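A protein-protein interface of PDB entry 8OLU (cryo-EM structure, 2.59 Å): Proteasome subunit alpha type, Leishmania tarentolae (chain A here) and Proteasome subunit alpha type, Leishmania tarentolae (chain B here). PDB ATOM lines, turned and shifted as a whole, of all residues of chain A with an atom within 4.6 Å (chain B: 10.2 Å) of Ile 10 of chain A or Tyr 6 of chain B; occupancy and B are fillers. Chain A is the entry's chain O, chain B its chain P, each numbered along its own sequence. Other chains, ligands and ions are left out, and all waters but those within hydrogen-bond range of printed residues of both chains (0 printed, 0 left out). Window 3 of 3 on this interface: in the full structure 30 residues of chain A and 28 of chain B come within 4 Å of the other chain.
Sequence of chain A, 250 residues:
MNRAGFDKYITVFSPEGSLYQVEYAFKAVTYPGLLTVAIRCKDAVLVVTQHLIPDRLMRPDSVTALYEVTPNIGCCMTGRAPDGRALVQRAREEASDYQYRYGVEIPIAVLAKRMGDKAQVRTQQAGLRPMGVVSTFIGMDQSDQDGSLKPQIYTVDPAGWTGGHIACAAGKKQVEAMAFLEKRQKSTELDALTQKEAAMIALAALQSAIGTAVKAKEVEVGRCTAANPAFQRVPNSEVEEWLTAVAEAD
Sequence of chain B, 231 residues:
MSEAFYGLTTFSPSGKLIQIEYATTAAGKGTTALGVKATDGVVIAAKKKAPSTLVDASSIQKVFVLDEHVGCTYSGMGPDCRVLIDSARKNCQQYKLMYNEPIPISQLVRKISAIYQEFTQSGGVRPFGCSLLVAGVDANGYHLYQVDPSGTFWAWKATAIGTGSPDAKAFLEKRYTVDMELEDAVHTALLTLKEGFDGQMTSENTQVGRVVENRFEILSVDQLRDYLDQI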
ATOM      1  N   PHE A   6     -30.762  -7.460 -12.350  1.00  0.00           N
ATOM      2  CA  PHE A   6     -29.730  -6.442 -12.691  1.00  0.00           C
ATOM      3  C   PHE A   6     -29.307  -6.569 -14.150  1.00  0.00           C
ATOM      4  O   PHE A   6     -28.987  -5.577 -14.795  1.00  0.00           O
ATOM      5  CB  PHE A   6     -28.503  -6.576 -11.785  1.00  0.00           C
ATOM      6  CG  PHE A   6     -27.480  -5.471 -11.945  1.00  0.00           C
ATOM      7  CD1 PHE A   6     -27.438  -4.405 -11.047  1.00  0.00           C
ATOM      8  CD2 PHE A   6     -26.539  -5.506 -12.974  1.00  0.00           C
ATOM      9  CE1 PHE A   6     -26.495  -3.395 -11.182  1.00  0.00           C
ATOM     10  CE2 PHE A   6     -25.594  -4.496 -13.109  1.00  0.00           C
ATOM     11  CZ  PHE A   6     -25.572  -3.445 -12.210  1.00  0.00           C
ATOM     12  N   ASP A   7     -29.289  -7.811 -14.643  1.00  0.00           N
ATOM     13  CA  ASP A   7     -28.970  -8.133 -16.029  1.00  0.00           C
ATOM     14  C   ASP A   7     -30.222  -8.092 -16.893  1.00  0.00           C
ATOM     15  O   ASP A   7     -30.114  -8.210 -18.101  1.00  0.00           O
ATOM     16  CB  ASP A   7     -28.303  -9.518 -16.149  1.00  0.00           C
ATOM     17  CG  ASP A   7     -29.031 -10.677 -15.478  1.00  0.00           C
ATOM     18  OD1 ASP A   7     -30.226 -10.553 -15.233  1.00  0.00           O
ATOM     19  OD2 ASP A   7     -28.383 -11.704 -15.175  1.00  0.00           O
ATOM     20  N   LYS A   8     -31.409  -7.994 -16.289  1.00  0.00           N
ATOM     21  CA  LYS A   8     -32.644  -8.124 -17.046  1.00  0.00           C
ATOM     22  C   LYS A   8     -32.979  -6.786 -17.697  1.00  0.00           C
ATOM     23  O   LYS A   8     -33.725  -6.741 -18.670  1.00  0.00           O
ATOM     24  CB  LYS A   8     -33.781  -8.643 -16.167  1.00  0.00           C
ATOM     25  CG  LYS A   8     -33.672 -10.107 -15.768  1.00  0.00           C
ATOM     26  CD  LYS A   8     -34.756 -10.546 -14.788  1.00  0.00           C
ATOM     27  CE  LYS A   8     -34.503 -11.917 -14.191  1.00  0.00           C
ATOM     28  NZ  LYS A   8     -34.199 -12.924 -15.238  1.00  0.00           N
ATOM     29  N   TYR A   9     -32.346  -5.729 -17.196  1.00  0.00           N
ATOM     30  CA  TYR A   9     -32.716  -4.372 -17.503  1.00  0.00           C
ATOM     31  C   TYR A   9     -31.584  -3.643 -18.212  1.00  0.00           C
ATOM     32  O   TYR A   9     -31.711  -2.490 -18.594  1.00  0.00           O
ATOM     33  CB  TYR A   9     -33.071  -3.602 -16.230  1.00  0.00           C
ATOM     34  CG  TYR A   9     -33.848  -4.345 -15.171  1.00  0.00           C
ATOM     35  CD1 TYR A   9     -35.019  -5.050 -15.471  1.00  0.00           C
ATOM     36  CD2 TYR A   9     -33.384  -4.343 -13.855  1.00  0.00           C
ATOM     37  CE1 TYR A   9     -35.707  -5.733 -14.473  1.00  0.00           C
ATOM     38  CE2 TYR A   9     -34.060  -5.019 -12.851  1.00  0.00           C
ATOM     39  CZ  TYR A   9     -35.227  -5.706 -13.161  1.00  0.00           C
ATOM     40  OH  TYR A   9     -35.865  -6.352 -12.127  1.00  0.00           O
ATOM     41  N   ILE A  10     -30.458  -4.282 -18.415  1.00  0.00           N
ATOM     42  CA  ILE A  10     -29.443  -3.569 -19.140  1.00  0.00           C
ATOM     43  C   ILE A  10     -28.760  -4.556 -20.072  1.00  0.00           C
ATOM     44  O   ILE A  10     -28.961  -5.754 -19.998  1.00  0.00           O
ATOM     45  CB  ILE A  10     -28.520  -2.823 -18.143  1.00  0.00           C
ATOM     46  CG1 ILE A  10     -27.879  -1.571 -18.752  1.00  0.00           C
ATOM     47  CG2 ILE A  10     -27.491  -3.735 -17.481  1.00  0.00           C
ATOM     48  CD1 ILE A  10     -26.496  -1.246 -18.181  1.00  0.00           C
ATOM     49  N   THR A  11     -28.004  -4.034 -21.005  1.00  0.00           N
ATOM     50  CA  THR A  11     -27.489  -4.880 -22.036  1.00  0.00           C
ATOM     51  C   THR A  11     -26.150  -5.455 -21.568  1.00  0.00           C
ATOM     52  O   THR A  11     -25.090  -5.151 -22.087  1.00  0.00           O
ATOM     53  CB  THR A  11     -27.485  -4.063 -23.333  1.00  0.00           C
ATOM     54  OG1 THR A  11     -27.792  -4.943 -24.431  1.00  0.00           O
ATOM     55  CG2 THR A  11     -26.184  -3.274 -23.477  1.00  0.00           C
ATOM     56  N   VAL A  12     -26.214  -6.297 -20.555  1.00  0.00           N
ATOM     57  CA  VAL A  12     -25.087  -7.094 -20.118  1.00  0.00           C
ATOM     58  C   VAL A  12     -25.537  -8.526 -20.198  1.00  0.00           C
ATOM     59  O   VAL A  12     -26.728  -8.778 -20.269  1.00  0.00           O
ATOM     60  CB  VAL A  12     -24.702  -6.795 -18.668  1.00  0.00           C
ATOM     61  CG1 VAL A  12     -24.243  -5.365 -18.539  1.00  0.00           C
ATOM     62  CG2 VAL A  12     -25.850  -7.089 -17.732  1.00  0.00           C
ATOM     63  N   GLN A  21     -32.474  -8.279 -22.554  1.00  0.00           N
ATOM     64  CA  GLN A  21     -33.198  -7.202 -23.187  1.00  0.00           C
ATOM     65  C   GLN A  21     -33.352  -7.535 -24.651  1.00  0.00           C
ATOM     66  O   GLN A  21     -34.405  -7.281 -25.204  1.00  0.00           O
ATOM     67  CB  GLN A  21     -32.545  -5.843 -22.983  1.00  0.00           C
ATOM     68  CG  GLN A  21     -32.866  -5.245 -21.620  1.00  0.00           C
ATOM     69  CD  GLN A  21     -34.332  -4.909 -21.536  1.00  0.00           C
ATOM     70  OE1 GLN A  21     -34.823  -4.206 -22.403  1.00  0.00           O
ATOM     71  NE2 GLN A  21     -35.057  -5.478 -20.592  1.00  0.00           N
ATOM     72  N   ALA A 126     -25.025   0.377 -23.564  1.00  0.00           N
ATOM     73  CA  ALA A 126     -26.115   0.368 -22.593  1.00  0.00           C
ATOM     74  C   ALA A 126     -27.044   1.568 -22.702  1.00  0.00           C
ATOM     75  O   ALA A 126     -26.648   2.680 -23.060  1.00  0.00           O
ATOM     76  CB  ALA A 126     -25.564   0.364 -21.201  1.00  0.00           C
ATOM     77  N   GLU B   3     -24.411   7.330 -24.142  1.00  0.00           N
ATOM     78  CA  GLU B   3     -24.378   8.354 -23.057  1.00  0.00           C
ATOM     79  C   GLU B   3     -24.188   7.681 -21.681  1.00  0.00           C
ATOM     80  O   GLU B   3     -24.111   8.403 -20.678  1.00  0.00           O
ATOM     81  CB  GLU B   3     -25.634   9.257 -23.120  1.00  0.00           C
ATOM     82  CG  GLU B   3     -25.518  10.564 -22.307  1.00  0.00           C
ATOM     83  CD  GLU B   3     -26.773  11.393 -22.036  1.00  0.00           C
ATOM     84  OE1 GLU B   3     -27.452  11.801 -23.024  1.00  0.00           O
ATOM     85  OE2 GLU B   3     -27.043  11.683 -20.833  1.00  0.00           O
ATOM     86  N   ALA B   4     -24.124   6.327 -21.598  1.00  0.00           N
ATOM     87  CA  ALA B   4     -23.726   5.661 -20.353  1.00  0.00           C
ATOM     88  C   ALA B   4     -22.220   5.457 -20.370  1.00  0.00           C
ATOM     89  O   ALA B   4     -21.674   4.974 -21.346  1.00  0.00           O
ATOM     90  CB  ALA B   4     -24.412   4.353 -20.133  1.00  0.00           C
ATOM     91  N   PHE B   5     -21.530   5.938 -19.347  1.00  0.00           N
ATOM     92  CA  PHE B   5     -20.091   5.978 -19.464  1.00  0.00           C
ATOM     93  C   PHE B   5     -19.437   5.201 -18.343  1.00  0.00           C
ATOM     94  O   PHE B   5     -18.208   5.147 -18.274  1.00  0.00           O
ATOM     95  CB  PHE B   5     -19.570   7.411 -19.412  1.00  0.00           C
ATOM     96  CG  PHE B   5     -19.708   8.178 -20.689  1.00  0.00           C
ATOM     97  CD1 PHE B   5     -18.839   7.946 -21.741  1.00  0.00           C
ATOM     98  CD2 PHE B   5     -20.703   9.142 -20.820  1.00  0.00           C
ATOM     99  CE1 PHE B   5     -18.987   8.654 -22.932  1.00  0.00           C
ATOM    100  CE2 PHE B   5     -20.858   9.839 -22.008  1.00  0.00           C
ATOM    101  CZ  PHE B   5     -19.999   9.594 -23.061  1.00  0.00           C
ATOM    102  N   TYR B   6     -20.240   4.675 -17.454  1.00  0.00           N
ATOM    103  CA  TYR B   6     -19.673   3.835 -16.448  1.00  0.00           C
ATOM    104  C   TYR B   6     -19.414   2.462 -17.013  1.00  0.00           C
ATOM    105  O   TYR B   6     -19.988   2.101 -18.025  1.00  0.00           O
ATOM    106  CB  TYR B   6     -20.612   3.726 -15.281  1.00  0.00           C
ATOM    107  CG  TYR B   6     -21.980   3.203 -15.592  1.00  0.00           C
ATOM    108  CD1 TYR B   6     -22.233   1.844 -15.686  1.00  0.00           C
ATOM    109  CD2 TYR B   6     -23.039   4.075 -15.686  1.00  0.00           C
ATOM    110  CE1 TYR B   6     -23.527   1.375 -15.835  1.00  0.00           C
ATOM    111  CE2 TYR B   6     -24.330   3.625 -15.859  1.00  0.00           C
ATOM    112  CZ  TYR B   6     -24.578   2.275 -15.962  1.00  0.00           C
ATOM    113  OH  TYR B   6     -25.865   1.856 -16.170  1.00  0.00           O
ATOM    114  N   GLY B   7     -18.532   1.718 -16.378  1.00  0.00           N
ATOM    115  CA  GLY B   7     -18.162   0.422 -16.868  1.00  0.00           C
ATOM    116  C   GLY B   7     -19.144  -0.632 -16.408  1.00  0.00           C
ATOM    117  O   GLY B   7     -19.634  -0.530 -15.303  1.00  0.00           O
ATOM    118  N   LEU B   8     -19.354  -1.657 -17.254  1.00  0.00           N
ATOM    119  CA  LEU B   8     -20.312  -2.730 -17.015  1.00  0.00           C
ATOM    120  C   LEU B   8     -19.586  -3.984 -16.570  1.00  0.00           C
ATOM    121  O   LEU B   8     -20.094  -4.754 -15.743  1.00  0.00           O
ATOM    122  CB  LEU B   8     -21.078  -3.022 -18.305  1.00  0.00           C
ATOM    123  CG  LEU B   8     -21.867  -1.826 -18.845  1.00  0.00           C
ATOM    124  CD1 LEU B   8     -22.614  -2.160 -20.110  1.00  0.00           C
ATOM    125  CD2 LEU B   8     -22.834  -1.329 -17.782  1.00  0.00           C
ATOM    126  N   THR B   9     -18.380  -4.136 -17.099  1.00  0.00           N
ATOM    127  CA  THR B   9     -17.463  -5.165 -16.675  1.00  0.00           C
ATOM    128  C   THR B   9     -16.600  -4.591 -15.588  1.00  0.00           C
ATOM    129  O   THR B   9     -15.980  -3.553 -15.835  1.00  0.00           O
ATOM    130  CB  THR B   9     -16.540  -5.625 -17.795  1.00  0.00           C
ATOM    131  OG1 THR B   9     -17.319  -6.065 -18.914  1.00  0.00           O
ATOM    132  CG2 THR B   9     -15.593  -6.725 -17.379  1.00  0.00           C
ATOM    133  N   THR B  10     -16.630  -5.285 -14.430  1.00  0.00           N
ATOM    134  CA  THR B  10     -15.913  -4.917 -13.232  1.00  0.00           C
ATOM    135  C   THR B  10     -15.401  -6.128 -12.483  1.00  0.00           C
ATOM    136  O   THR B  10     -15.896  -7.225 -12.673  1.00  0.00           O
ATOM    137  CB  THR B  10     -16.819  -4.212 -12.236  1.00  0.00           C
ATOM    138  OG1 THR B  10     -17.920  -5.011 -11.791  1.00  0.00           O
ATOM    139  CG2 THR B  10     -17.332  -2.919 -12.826  1.00  0.00           C
ATOM    140  N   GLN B  19     -18.670 -10.403 -16.062  1.00  0.00           N
ATOM    141  CA  GLN B  19     -19.227 -10.192 -17.379  1.00  0.00           C
ATOM    142  C   GLN B  19     -18.396 -10.890 -18.439  1.00  0.00           C
ATOM    143  O   GLN B  19     -18.939 -11.324 -19.430  1.00  0.00           O
ATOM    144  CB  GLN B  19     -19.317  -8.730 -17.819  1.00  0.00           C
ATOM    145  CG  GLN B  19     -20.605  -8.033 -17.419  1.00  0.00           C
ATOM    146  CD  GLN B  19     -21.822  -8.861 -17.743  1.00  0.00           C
ATOM    147  OE1 GLN B  19     -22.178  -8.983 -18.907  1.00  0.00           O
ATOM    148  NE2 GLN B  19     -22.454  -9.436 -16.744  1.00  0.00           N
ATOM    149  N   GLU B 118     -10.905  -3.545 -25.295  1.00  0.00           N
ATOM    150  CA  GLU B 118     -11.609  -2.297 -25.060  1.00  0.00           C
ATOM    151  C   GLU B 118     -13.018  -2.600 -24.583  1.00  0.00           C
ATOM    152  O   GLU B 118     -13.474  -1.929 -23.686  1.00  0.00           O
ATOM    153  CB  GLU B 118     -11.965  -1.378 -26.212  1.00  0.00           C
ATOM    154  CG  GLU B 118     -10.835  -0.830 -27.046  1.00  0.00           C
ATOM    155  CD  GLU B 118     -11.353  -0.290 -28.402  1.00  0.00           C
ATOM    156  OE1 GLU B 118     -12.564   0.102 -28.497  1.00  0.00           O
ATOM    157  OE2 GLU B 118     -10.570  -0.307 -29.400  1.00  0.00           O
ATOM    158  N   PHE B 119     -13.718  -3.577 -25.130  1.00  0.00           N
ATOM    159  CA  PHE B 119     -15.076  -3.751 -24.671  1.00  0.00           C
ATOM    160  C   PHE B 119     -15.137  -4.440 -23.310  1.00  0.00           C
ATOM    161  O   PHE B 119     -16.219  -4.664 -22.804  1.00  0.00           O
ATOM    162  CB  PHE B 119     -15.936  -4.421 -25.727  1.00  0.00           C
ATOM    163  CG  PHE B 119     -16.331  -3.479 -26.838  1.00  0.00           C
ATOM    164  CD1 PHE B 119     -17.631  -3.031 -26.968  1.00  0.00           C
ATOM    165  CD2 PHE B 119     -15.393  -3.022 -27.758  1.00  0.00           C
ATOM    166  CE1 PHE B 119     -17.973  -2.147 -27.988  1.00  0.00           C
ATOM    167  CE2 PHE B 119     -15.719  -2.122 -28.760  1.00  0.00           C
ATOM    168  CZ  PHE B 119     -17.019  -1.697 -28.883  1.00  0.00           C
ATOM    169  N   THR B 120     -14.002  -4.669 -22.641  1.00  0.00           N
ATOM    170  CA  THR B 120     -14.005  -5.246 -21.304  1.00  0.00           C
ATOM    171  C   THR B 120     -13.711  -4.174 -20.261  1.00  0.00           C
ATOM    172  O   THR B 120     -13.552  -4.477 -19.089  1.00  0.00           O
ATOM    173  CB  THR B 120     -12.916  -6.323 -21.161  1.00  0.00           C
ATOM    174  OG1 THR B 120     -11.604  -5.763 -21.255  1.00  0.00           O
ATOM    175  CG2 THR B 120     -13.008  -7.390 -22.221  1.00  0.00           C
ATOM    176  N   GLN B 121     -13.494  -2.950 -20.719  1.00  0.00           N
ATOM    177  CA  GLN B 121     -13.023  -1.916 -19.827  1.00  0.00           C
ATOM    178  C   GLN B 121     -13.756  -0.617 -20.105  1.00  0.00           C
ATOM    179  O   GLN B 121     -14.256  -0.037 -19.164  1.00  0.00           O
ATOM    180  CB  GLN B 121     -11.515  -1.724 -20.001  1.00  0.00           C
ATOM    181  CG  GLN B 121     -10.877  -0.672 -19.099  1.00  0.00           C
ATOM    182  CD  GLN B 121      -9.438  -1.022 -18.843  1.00  0.00           C
ATOM    183  OE1 GLN B 121      -8.710  -1.361 -19.772  1.00  0.00           O
ATOM    184  NE2 GLN B 121      -9.034  -1.012 -17.583  1.00  0.00           N
ATOM    185  N   SER B 122     -13.799  -0.172 -21.359  1.00  0.00           N
ATOM    186  CA  SER B 122     -14.545   1.007 -21.766  1.00  0.00           C
ATOM    187  C   SER B 122     -15.923   1.050 -21.156  1.00  0.00           C
ATOM    188  O   SER B 122     -16.533   0.018 -20.907  1.00  0.00           O
ATOM    189  CB  SER B 122     -14.747   1.098 -23.261  1.00  0.00           C
ATOM    190  OG  SER B 122     -13.786   1.968 -23.829  1.00  0.00           O
ATOM    191  N   GLY B 123     -16.428   2.269 -21.055  1.00  0.00           N
ATOM    192  CA  GLY B 123     -17.699   2.481 -20.396  1.00  0.00           C
ATOM    193  C   GLY B 123     -18.871   2.261 -21.325  1.00  0.00           C
ATOM    194  O   GLY B 123     -18.774   2.420 -22.532  1.00  0.00           O
ATOM    195  N   GLY B 124     -19.948   1.817 -20.719  1.00  0.00           N
ATOM    196  CA  GLY B 124     -21.190   1.655 -21.439  1.00  0.00           C
ATOM    197  C   GLY B 124     -21.345   0.341 -22.185  1.00  0.00           C
ATOM    198  O   GLY B 124     -22.426  -0.015 -22.567  1.00  0.00           O
ATOM    199  N   VAL B 125     -20.310  -0.429 -22.381  1.00  0.00           N
ATOM    200  CA  VAL B 125     -20.445  -1.505 -23.320  1.00  0.00           C
ATOM    201  C   VAL B 125     -20.305  -2.795 -22.577  1.00  0.00           C
ATOM    202  O   VAL B 125     -19.702  -2.813 -21.527  1.00  0.00           O
ATOM    203  CB  VAL B 125     -19.361  -1.394 -24.371  1.00  0.00           C
ATOM    204  CG1 VAL B 125     -19.616  -0.197 -25.294  1.00  0.00           C
ATOM    205  CG2 VAL B 125     -18.007  -1.272 -23.706  1.00  0.00           C
ATOM    206  N   ARG B 126     -20.912  -3.839 -23.094  1.00  0.00           N
ATOM    207  CA  ARG B 126     -20.644  -5.150 -22.574  1.00  0.00           C
ATOM    208  C   ARG B 126     -19.565  -5.737 -23.455  1.00  0.00           C
ATOM    209  O   ARG B 126     -19.408  -5.317 -24.574  1.00  0.00           O
ATOM    210  CB  ARG B 126     -21.894  -6.027 -22.670  1.00  0.00           C
ATOM    211  CG  ARG B 126     -22.367  -6.239 -24.090  1.00  0.00           C
ATOM    212  CD  ARG B 126     -23.281  -7.403 -24.151  1.00  0.00           C
ATOM    213  NE  ARG B 126     -23.991  -7.392 -25.437  1.00  0.00           N
ATOM    214  CZ  ARG B 126     -23.463  -7.731 -26.611  1.00  0.00           C
ATOM    215  NH1 ARG B 126     -24.133  -7.518 -27.721  1.00  0.00           N
ATOM    216  NH2 ARG B 126     -22.268  -8.284 -26.661  1.00  0.00           N
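The backbone NH (N) of Ala 126 of chain A sits at hydrogen-bond distance from the backbone carbonyl oxygen (O) of Gly 124 of chain B, at 2.8 Å.
The backbone carbonyl oxygen (O) of Tyr 6 of chain B sits at hydrogen-bond distance from the backbone NH (N) of Gly 124 of chain B (2.7 Å).
OH of Tyr 6 of chain B touches CD1 of Ile 10 of chain A, 3.8 Å away. Leu 8 of chain B touches Ile 10 of chain A. O of Thr 11 of chain A touches CB of Arg 126 of chain B (3.4 Å). Val 12 of chain A touches Leu 8 of chain B. Val 12 of chain A touches Gln 19 of chain B (CB to OE1, 3.3 Å).
Ile 10 of chain A touches two residues of chain B. Tyr 6 of chain B touches one residue of chain A. Thr 11 of chain A touches one residue of chain B. Val 12 of chain A touches just these residues of chain B: Leu 8 (3.9 Å) and Gln 19 (3.3 Å). Printed residues of chain A within 4 Å of Gly 124 of chain B: Ala 126. Printed residues of chain B within 4 Å of Ala 126 of chain A: Gly 124 (2.8 Å). Printed residues of chain A within 4 Å of Leu 8 of chain B: Ile 10 and Val 12. Of the printed residues of chain A, Gln 19 of chain B touches Val 12 (3.3 Å). Printed residues of chain A within 4 Å of Arg 126 of chain B: Thr 11 (3.4 Å). The nearest printed residue of chain A that does not touch Tyr 6 of chain B is Ala 126 of chain A (5.3 Å).
Hydrophobic or aromatic side chains of chain B that line the printed part of chain A: Tyr 6 and Leu 8. Along chain B the printed residues that touch a printed residue of chain A span positions 6 to 126. Hydrophobic or aromatic side chains of chain A that line the printed part of chain B: Ile 10, Val 12 and Ala 126. Among the printed residues, 6 pairs touch across the chains.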
